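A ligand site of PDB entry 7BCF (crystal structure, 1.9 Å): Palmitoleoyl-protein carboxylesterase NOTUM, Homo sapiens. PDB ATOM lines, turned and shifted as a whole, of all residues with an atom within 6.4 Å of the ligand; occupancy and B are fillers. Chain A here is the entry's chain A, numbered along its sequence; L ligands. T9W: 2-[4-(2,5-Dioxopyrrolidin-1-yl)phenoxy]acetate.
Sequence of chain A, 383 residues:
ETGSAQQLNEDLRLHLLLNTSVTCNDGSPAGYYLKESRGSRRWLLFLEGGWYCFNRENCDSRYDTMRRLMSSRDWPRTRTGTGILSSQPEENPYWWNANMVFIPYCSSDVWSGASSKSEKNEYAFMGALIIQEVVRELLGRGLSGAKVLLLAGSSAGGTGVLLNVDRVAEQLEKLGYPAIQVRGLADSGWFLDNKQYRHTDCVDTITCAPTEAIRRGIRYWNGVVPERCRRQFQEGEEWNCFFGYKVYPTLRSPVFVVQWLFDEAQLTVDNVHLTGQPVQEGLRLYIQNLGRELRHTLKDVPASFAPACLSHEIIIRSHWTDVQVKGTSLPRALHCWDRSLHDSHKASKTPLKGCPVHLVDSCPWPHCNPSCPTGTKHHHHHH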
ATOM      1  N   GLY A  49     -14.981  16.240 -18.650  1.00  0.00           N
ATOM      2  CA  GLY A  49     -14.534  16.644 -17.342  1.00  0.00           C
ATOM      3  C   GLY A  49     -15.222  17.915 -16.862  1.00  0.00           C
ATOM      4  O   GLY A  49     -16.183  18.395 -17.461  1.00  0.00           O
ATOM      5  N   GLY A  50     -14.726  18.444 -15.735  1.00  0.00           N
ATOM      6  CA  GLY A  50     -15.189  19.720 -15.194  1.00  0.00           C
ATOM      7  C   GLY A  50     -15.330  19.767 -13.680  1.00  0.00           C
ATOM      8  O   GLY A  50     -16.377  20.182 -13.178  1.00  0.00           O
ATOM      9  N   TRP A  51     -14.297  19.352 -12.949  1.00  0.00           N
ATOM     10  CA  TRP A  51     -14.211  19.385 -11.461  1.00  0.00           C
ATOM     11  C   TRP A  51     -15.363  18.552 -10.872  1.00  0.00           C
ATOM     12  O   TRP A  51     -15.634  17.443 -11.390  1.00  0.00           O
ATOM     13  CB  TRP A  51     -14.151  20.817 -10.960  1.00  0.00           C
ATOM     14  CG  TRP A  51     -12.829  21.467 -11.284  1.00  0.00           C
ATOM     15  CD1 TRP A  51     -12.574  22.336 -12.305  1.00  0.00           C
ATOM     16  CD2 TRP A  51     -11.594  21.298 -10.585  1.00  0.00           C
ATOM     17  NE1 TRP A  51     -11.240  22.710 -12.283  1.00  0.00           N
ATOM     18  CE2 TRP A  51     -10.626  22.075 -11.237  1.00  0.00           C
ATOM     19  CE3 TRP A  51     -11.209  20.558  -9.460  1.00  0.00           C
ATOM     20  CZ2 TRP A  51      -9.292  22.148 -10.798  1.00  0.00           C
ATOM     21  CZ3 TRP A  51      -9.891  20.621  -9.032  1.00  0.00           C
ATOM     22  CH2 TRP A  51      -8.951  21.406  -9.705  1.00  0.00           C
ATOM     23  N   TYR A  52     -16.012  19.037  -9.806  1.00  0.00           N
ATOM     24  CA  TYR A  52     -17.042  18.324  -9.032  1.00  0.00           C
ATOM     25  C   TYR A  52     -17.553  19.258  -7.925  1.00  0.00           C
ATOM     26  O   TYR A  52     -17.011  20.342  -7.699  1.00  0.00           O
ATOM     27  CB  TYR A  52     -16.505  17.025  -8.435  1.00  0.00           C
ATOM     28  CG  TYR A  52     -15.385  17.204  -7.425  1.00  0.00           C
ATOM     29  CD1 TYR A  52     -15.653  17.278  -6.059  1.00  0.00           C
ATOM     30  CD2 TYR A  52     -14.064  17.287  -7.834  1.00  0.00           C
ATOM     31  CE1 TYR A  52     -14.616  17.437  -5.126  1.00  0.00           C
ATOM     32  CE2 TYR A  52     -13.024  17.453  -6.922  1.00  0.00           C
ATOM     33  CZ  TYR A  52     -13.308  17.523  -5.574  1.00  0.00           C
ATOM     34  OH  TYR A  52     -12.244  17.689  -4.716  1.00  0.00           O
ATOM     35  N   TYR A 105     -20.874  15.452 -18.965  1.00  0.00           N
ATOM     36  CA  TYR A 105     -20.666  15.337 -17.523  1.00  0.00           C
ATOM     37  C   TYR A 105     -21.724  16.181 -16.820  1.00  0.00           C
ATOM     38  O   TYR A 105     -21.630  17.419 -16.807  1.00  0.00           O
ATOM     39  CB  TYR A 105     -19.257  15.798 -17.174  1.00  0.00           C
ATOM     40  CG  TYR A 105     -18.801  15.696 -15.731  1.00  0.00           C
ATOM     41  CD1 TYR A 105     -19.193  14.639 -14.919  1.00  0.00           C
ATOM     42  CD2 TYR A 105     -17.934  16.654 -15.191  1.00  0.00           C
ATOM     43  CE1 TYR A 105     -18.732  14.550 -13.600  1.00  0.00           C
ATOM     44  CE2 TYR A 105     -17.468  16.551 -13.885  1.00  0.00           C
ATOM     45  CZ  TYR A 105     -17.868  15.506 -13.089  1.00  0.00           C
ATOM     46  OH  TYR A 105     -17.403  15.424 -11.791  1.00  0.00           O
ATOM     47  N   VAL A 110     -17.178  13.035 -10.340  1.00  0.00           N
ATOM     48  CA  VAL A 110     -15.999  12.427 -10.942  1.00  0.00           C
ATOM     49  C   VAL A 110     -16.396  11.069 -11.532  1.00  0.00           C
ATOM     50  O   VAL A 110     -15.584  10.129 -11.593  1.00  0.00           O
ATOM     51  CB  VAL A 110     -14.850  12.354  -9.903  1.00  0.00           C
ATOM     52  CG1 VAL A 110     -13.565  11.772 -10.488  1.00  0.00           C
ATOM     53  CG2 VAL A 110     -14.625  13.729  -9.172  1.00  0.00           C
ATOM     54  N   SER A 154     -11.226  13.118 -20.234  1.00  0.00           N
ATOM     55  CA  SER A 154     -10.270  14.192 -19.989  1.00  0.00           C
ATOM     56  C   SER A 154     -10.538  14.841 -18.626  1.00  0.00           C
ATOM     57  O   SER A 154     -11.686  15.189 -18.314  1.00  0.00           O
ATOM     58  CB  SER A 154     -10.345  15.252 -21.087  1.00  0.00           C
ATOM     59  OG  SER A 154      -9.726  14.818 -22.286  1.00  0.00           O
ATOM     60  N   SER A 155      -9.476  15.031 -17.827  1.00  0.00           N
ATOM     61  CA  SER A 155      -9.520  15.761 -16.551  1.00  0.00           C
ATOM     62  C   SER A 155     -10.317  14.929 -15.559  1.00  0.00           C
ATOM     63  O   SER A 155      -9.959  13.762 -15.328  1.00  0.00           O
ATOM     64  CB  SER A 155     -10.053  17.180 -16.766  1.00  0.00           C
ATOM     65  OG  SER A 155      -9.207  17.938 -17.592  1.00  0.00           O
ATOM     66  N   ALA A 156     -11.412  15.456 -14.985  1.00  0.00           N
ATOM     67  CA  ALA A 156     -12.267  14.595 -14.172  1.00  0.00           C
ATOM     68  C   ALA A 156     -12.791  13.402 -14.972  1.00  0.00           C
ATOM     69  O   ALA A 156     -13.042  12.337 -14.403  1.00  0.00           O
ATOM     70  CB  ALA A 156     -13.451  15.379 -13.598  1.00  0.00           C
ATOM     71  N   GLY A 157     -12.990  13.585 -16.283  1.00  0.00           N
ATOM     72  CA  GLY A 157     -13.384  12.448 -17.105  1.00  0.00           C
ATOM     73  C   GLY A 157     -12.276  11.415 -17.246  1.00  0.00           C
ATOM     74  O   GLY A 157     -12.552  10.229 -17.413  1.00  0.00           O
ATOM     75  N   THR A 159     -10.033  10.734 -14.779  1.00  0.00           N
ATOM     76  CA  THR A 159     -10.140   9.941 -13.558  1.00  0.00           C
ATOM     77  C   THR A 159     -11.320   8.963 -13.634  1.00  0.00           C
ATOM     78  O   THR A 159     -11.232   7.825 -13.163  1.00  0.00           O
ATOM     79  CB  THR A 159     -10.289  10.864 -12.342  1.00  0.00           C
ATOM     80  OG1 THR A 159      -9.211  11.813 -12.341  1.00  0.00           O
ATOM     81  CG2 THR A 159     -10.209  10.086 -11.041  1.00  0.00           C
ATOM     82  N   SER A 188      -5.155  13.483 -18.598  1.00  0.00           N
ATOM     83  CA  SER A 188      -5.087  14.558 -17.583  1.00  0.00           C
ATOM     84  C   SER A 188      -5.874  14.215 -16.305  1.00  0.00           C
ATOM     85  O   SER A 188      -6.346  15.106 -15.602  1.00  0.00           O
ATOM     86  CB  SER A 188      -5.584  15.893 -18.157  1.00  0.00           C
ATOM     87  OG  SER A 188      -4.778  16.332 -19.237  1.00  0.00           O
ATOM     88  N   GLY A 189      -5.996  12.925 -15.974  1.00  0.00           N
ATOM     89  CA  GLY A 189      -6.680  12.545 -14.750  1.00  0.00           C
ATOM     90  C   GLY A 189      -5.829  11.789 -13.732  1.00  0.00           C
ATOM     91  O   GLY A 189      -6.365  11.070 -12.877  1.00  0.00           O
ATOM     92  N   PHE A 191      -3.478  12.242 -10.831  1.00  0.00           N
ATOM     93  CA  PHE A 191      -3.144  13.252  -9.830  1.00  0.00           C
ATOM     94  C   PHE A 191      -2.335  12.657  -8.667  1.00  0.00           C
ATOM     95  O   PHE A 191      -2.341  11.446  -8.405  1.00  0.00           O
ATOM     96  CB  PHE A 191      -4.401  13.931  -9.263  1.00  0.00           C
ATOM     97  CG  PHE A 191      -5.263  14.605 -10.304  1.00  0.00           C
ATOM     98  CD1 PHE A 191      -6.436  14.004 -10.753  1.00  0.00           C
ATOM     99  CD2 PHE A 191      -4.890  15.814 -10.842  1.00  0.00           C
ATOM    100  CE1 PHE A 191      -7.230  14.608 -11.717  1.00  0.00           C
ATOM    101  CE2 PHE A 191      -5.683  16.432 -11.820  1.00  0.00           C
ATOM    102  CZ  PHE A 191      -6.857  15.818 -12.255  1.00  0.00           C
ATOM    103  N   LEU A 192      -1.655  13.547  -7.944  1.00  0.00           N
ATOM    104  CA  LEU A 192      -0.819  13.185  -6.810  1.00  0.00           C
ATOM    105  C   LEU A 192      -1.402  13.795  -5.543  1.00  0.00           C
ATOM    106  O   LEU A 192      -1.833  14.952  -5.543  1.00  0.00           O
ATOM    107  CB  LEU A 192       0.625  13.678  -6.999  1.00  0.00           C
ATOM    108  CG  LEU A 192       1.413  13.205  -8.222  1.00  0.00           C
ATOM    109  CD1 LEU A 192       2.846  13.749  -8.174  1.00  0.00           C
ATOM    110  CD2 LEU A 192       1.410  11.665  -8.342  1.00  0.00           C
ATOM    111  N   PRO A 210      -7.690  18.699  -1.053  1.00  0.00           N
ATOM    112  CA  PRO A 210      -8.418  17.836  -2.000  1.00  0.00           C
ATOM    113  C   PRO A 210      -8.745  16.493  -1.418  1.00  0.00           C
ATOM    114  O   PRO A 210      -9.800  15.922  -1.723  1.00  0.00           O
ATOM    115  CB  PRO A 210      -7.433  17.694  -3.164  1.00  0.00           C
ATOM    116  CG  PRO A 210      -6.694  18.976  -3.138  1.00  0.00           C
ATOM    117  CD  PRO A 210      -6.495  19.292  -1.682  1.00  0.00           C
ATOM    118  N   THR A 211      -7.879  15.965  -0.555  1.00  0.00           N
ATOM    119  CA  THR A 211      -8.225  14.676   0.021  1.00  0.00           C
ATOM    120  C   THR A 211      -9.464  14.714   0.925  1.00  0.00           C
ATOM    121  O   THR A 211     -10.173  13.676   0.934  1.00  0.00           O
ATOM    122  CB  THR A 211      -7.072  14.000   0.752  1.00  0.00           C
ATOM    123  OG1 THR A 211      -6.590  14.843   1.786  1.00  0.00           O
ATOM    124  CG2 THR A 211      -5.871  13.709  -0.196  1.00  0.00           C
ATOM    125  N   ILE A 214     -12.589  15.029  -1.581  1.00  0.00           N
ATOM    126  CA  ILE A 214     -12.930  13.750  -2.204  1.00  0.00           C
ATOM    127  C   ILE A 214     -13.570  12.817  -1.185  1.00  0.00           C
ATOM    128  O   ILE A 214     -14.590  12.189  -1.459  1.00  0.00           O
ATOM    129  CB  ILE A 214     -11.670  13.118  -2.823  1.00  0.00           C
ATOM    130  CG1 ILE A 214     -11.138  13.995  -3.967  1.00  0.00           C
ATOM    131  CG2 ILE A 214     -11.986  11.702  -3.312  1.00  0.00           C
ATOM    132  CD1 ILE A 214     -11.970  13.926  -5.224  1.00  0.00           C
ATOM    133  N   TRP A 239     -11.224   6.798  -0.884  1.00  0.00           N
ATOM    134  CA  TRP A 239     -10.728   7.998  -1.545  1.00  0.00           C
ATOM    135  C   TRP A 239      -9.367   7.762  -2.188  1.00  0.00           C
ATOM    136  O   TRP A 239      -9.031   8.461  -3.155  1.00  0.00           O
ATOM    137  CB  TRP A 239     -10.650   9.173  -0.559  1.00  0.00           C
ATOM    138  CG  TRP A 239      -9.649   8.975   0.587  1.00  0.00           C
ATOM    139  CD1 TRP A 239      -9.932   8.528   1.842  1.00  0.00           C
ATOM    140  CD2 TRP A 239      -8.237   9.222   0.551  1.00  0.00           C
ATOM    141  NE1 TRP A 239      -8.766   8.481   2.608  1.00  0.00           N
ATOM    142  CE2 TRP A 239      -7.721   8.888   1.826  1.00  0.00           C
ATOM    143  CE3 TRP A 239      -7.356   9.695  -0.425  1.00  0.00           C
ATOM    144  CZ2 TRP A 239      -6.369   9.020   2.143  1.00  0.00           C
ATOM    145  CZ3 TRP A 239      -6.016   9.795  -0.124  1.00  0.00           C
ATOM    146  CH2 TRP A 239      -5.524   9.479   1.152  1.00  0.00           C
ATOM    147  N   PHE A 242      -9.092   7.202  -6.076  1.00  0.00           N
ATOM    148  CA  PHE A 242      -9.196   8.333  -7.015  1.00  0.00           C
ATOM    149  C   PHE A 242      -7.834   8.819  -7.514  1.00  0.00           C
ATOM    150  O   PHE A 242      -7.795   9.699  -8.375  1.00  0.00           O
ATOM    151  CB  PHE A 242      -9.926   9.514  -6.375  1.00  0.00           C
ATOM    152  CG  PHE A 242     -11.426   9.380  -6.364  1.00  0.00           C
ATOM    153  CD1 PHE A 242     -12.220  10.283  -7.068  1.00  0.00           C
ATOM    154  CD2 PHE A 242     -12.049   8.356  -5.658  1.00  0.00           C
ATOM    155  CE1 PHE A 242     -13.606  10.160  -7.067  1.00  0.00           C
ATOM    156  CE2 PHE A 242     -13.432   8.219  -5.656  1.00  0.00           C
ATOM    157  CZ  PHE A 242     -14.216   9.131  -6.365  1.00  0.00           C
ATOM    158  N   PHE A 243      -6.741   8.277  -6.990  1.00  0.00           N
ATOM    159  CA  PHE A 243      -5.396   8.666  -7.387  1.00  0.00           C
ATOM    160  C   PHE A 243      -4.809   7.586  -8.298  1.00  0.00           C
ATOM    161  O   PHE A 243      -4.642   6.429  -7.880  1.00  0.00           O
ATOM    162  CB  PHE A 243      -4.530   8.920  -6.149  1.00  0.00           C
ATOM    163  CG  PHE A 243      -4.974  10.136  -5.377  1.00  0.00           C
ATOM    164  CD1 PHE A 243      -5.995  10.046  -4.453  1.00  0.00           C
ATOM    165  CD2 PHE A 243      -4.405  11.378  -5.615  1.00  0.00           C
ATOM    166  CE1 PHE A 243      -6.423  11.153  -3.753  1.00  0.00           C
ATOM    167  CE2 PHE A 243      -4.832  12.492  -4.922  1.00  0.00           C
ATOM    168  CZ  PHE A 243      -5.843  12.382  -3.988  1.00  0.00           C
ATOM    169  N   ALA A 265      -4.423  21.686 -13.349  1.00  0.00           N
ATOM    170  CA  ALA A 265      -5.309  21.359 -12.241  1.00  0.00           C
ATOM    171  C   ALA A 265      -4.534  20.833 -11.030  1.00  0.00           C
ATOM    172  O   ALA A 265      -4.953  21.045  -9.885  1.00  0.00           O
ATOM    173  CB  ALA A 265      -6.362  20.325 -12.685  1.00  0.00           C
ATOM    174  N   VAL A 269      -4.669  22.604  -7.219  1.00  0.00           N
ATOM    175  CA  VAL A 269      -4.853  21.961  -5.919  1.00  0.00           C
ATOM    176  C   VAL A 269      -3.585  21.994  -5.074  1.00  0.00           C
ATOM    177  O   VAL A 269      -3.645  21.710  -3.872  1.00  0.00           O
ATOM    178  CB  VAL A 269      -5.366  20.520  -6.077  1.00  0.00           C
ATOM    179  CG1 VAL A 269      -6.704  20.487  -6.845  1.00  0.00           C
ATOM    180  CG2 VAL A 269      -4.345  19.645  -6.730  1.00  0.00           C
ATOM    181  N   HIS A 312      -3.377  21.588 -19.846  1.00  0.00           N
ATOM    182  CA  HIS A 312      -4.544  20.917 -19.273  1.00  0.00           C
ATOM    183  C   HIS A 312      -5.398  20.356 -20.411  1.00  0.00           C
ATOM    184  O   HIS A 312      -5.838  21.120 -21.274  1.00  0.00           O
ATOM    185  CB  HIS A 312      -5.351  21.906 -18.420  1.00  0.00           C
ATOM    186  CG  HIS A 312      -6.541  21.295 -17.753  1.00  0.00           C
ATOM    187  ND1 HIS A 312      -7.835  21.646 -18.072  1.00  0.00           N
ATOM    188  CD2 HIS A 312      -6.631  20.372 -16.771  1.00  0.00           C
ATOM    189  CE1 HIS A 312      -8.673  20.949 -17.326  1.00  0.00           C
ATOM    190  NE2 HIS A 312      -7.976  20.173 -16.525  1.00  0.00           N
ATOM    191  N   GLU A 313      -5.627  19.032 -20.403  1.00  0.00           N
ATOM    192  CA  GLU A 313      -6.356  18.285 -21.433  1.00  0.00           C
ATOM    193  C   GLU A 313      -5.618  18.284 -22.770  1.00  0.00           C
ATOM    194  O   GLU A 313      -4.744  19.134 -22.981  1.00  0.00           O
ATOM    195  CB  GLU A 313      -7.765  18.840 -21.640  1.00  0.00           C
ATOM    196  CG  GLU A 313      -8.628  18.754 -20.417  1.00  0.00           C
ATOM    197  CD  GLU A 313     -10.098  18.919 -20.728  1.00  0.00           C
ATOM    198  OE1 GLU A 313     -10.870  19.287 -19.803  1.00  0.00           O
ATOM    199  OE2 GLU A 313     -10.486  18.713 -21.905  1.00  0.00           O
HETATM  200  C10 T9W L   1      -8.286  13.103  -6.744  1.00  0.00           C
HETATM  201  C15 T9W L   1     -10.324  18.746 -12.880  1.00  0.00           C
HETATM  202  C01 T9W L   1     -10.830  15.513  -9.453  1.00  0.00           C
HETATM  203  C02 T9W L   1     -11.394  16.251 -10.482  1.00  0.00           C
HETATM  204  C03 T9W L   1     -10.667  17.281 -11.054  1.00  0.00           C
HETATM  205  C04 T9W L   1      -9.388  17.596 -10.614  1.00  0.00           C
HETATM  206  C05 T9W L   1      -8.827  16.865  -9.578  1.00  0.00           C
HETATM  207  C06 T9W L   1      -9.551  15.822  -9.005  1.00  0.00           C
HETATM  208  C08 T9W L   1      -9.012  13.542  -7.868  1.00  0.00           C
HETATM  209  C11 T9W L   1      -7.603  14.433  -6.106  1.00  0.00           C
HETATM  210  C12 T9W L   1      -8.125  15.547  -6.803  1.00  0.00           C
HETATM  211  C16 T9W L   1     -11.063  19.108 -14.157  1.00  0.00           C
HETATM  212  N07 T9W L   1      -8.946  15.042  -7.943  1.00  0.00           N
HETATM  213  O09 T9W L   1      -9.594  12.872  -8.655  1.00  0.00           O
HETATM  214  O13 T9W L   1      -7.969  16.691  -6.533  1.00  0.00           O
HETATM  215  O14 T9W L   1     -11.240  18.018 -12.086  1.00  0.00           O
HETATM  216  O17 T9W L   1     -10.683  20.091 -14.861  1.00  0.00           O
HETATM  217  O18 T9W L   1     -12.068  18.414 -14.491  1.00  0.00           O
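An oxygen (O17) of the ligand lies within hydrogen-bond range of a ring nitrogen (NE2) of His 312 (3.2 Å). N of Ala 156 lies within hydrogen-bond range of O18 of the ligand, 3.1 Å away. N of Gly 50 sits at hydrogen-bond distance from O18 of the ligand (2.9 Å). The backbone NH (N) of Trp 51 lies within hydrogen-bond range of an oxygen (O18) of the ligand (2.9 Å).
The side-chain hydroxyl of Ser 155 lies within hydrogen-bond range of a ring nitrogen (NE2) of His 312, at 2.8 Å. OE1 of Glu 313 sits close to OG of Ser 155 (3.1 Å). The backbone NH (N) of Gly 49 lies close to the backbone carbonyl oxygen (O) of Ser 154, at 3.5 Å. O of Trp 51 lies within hydrogen-bond range of OH of Tyr 105. The side-chain hydroxyl of Thr 159 is in hydrogen-bond range of the backbone carbonyl oxygen of Gly 189, at 3.0 Å.
Residues that only touch the ligand: Ser 155, Phe 243, Phe 191, Pro 210, Phe 242, Thr 159, Tyr 52, Gly 49 and Ile 214. Hydrophobic or aromatic side chains within 4 Å of the ligand: Trp 51, Tyr 52, Ala 156, Phe 191, Pro 210, Ile 214, Phe 242, Phe 243 and His 312.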
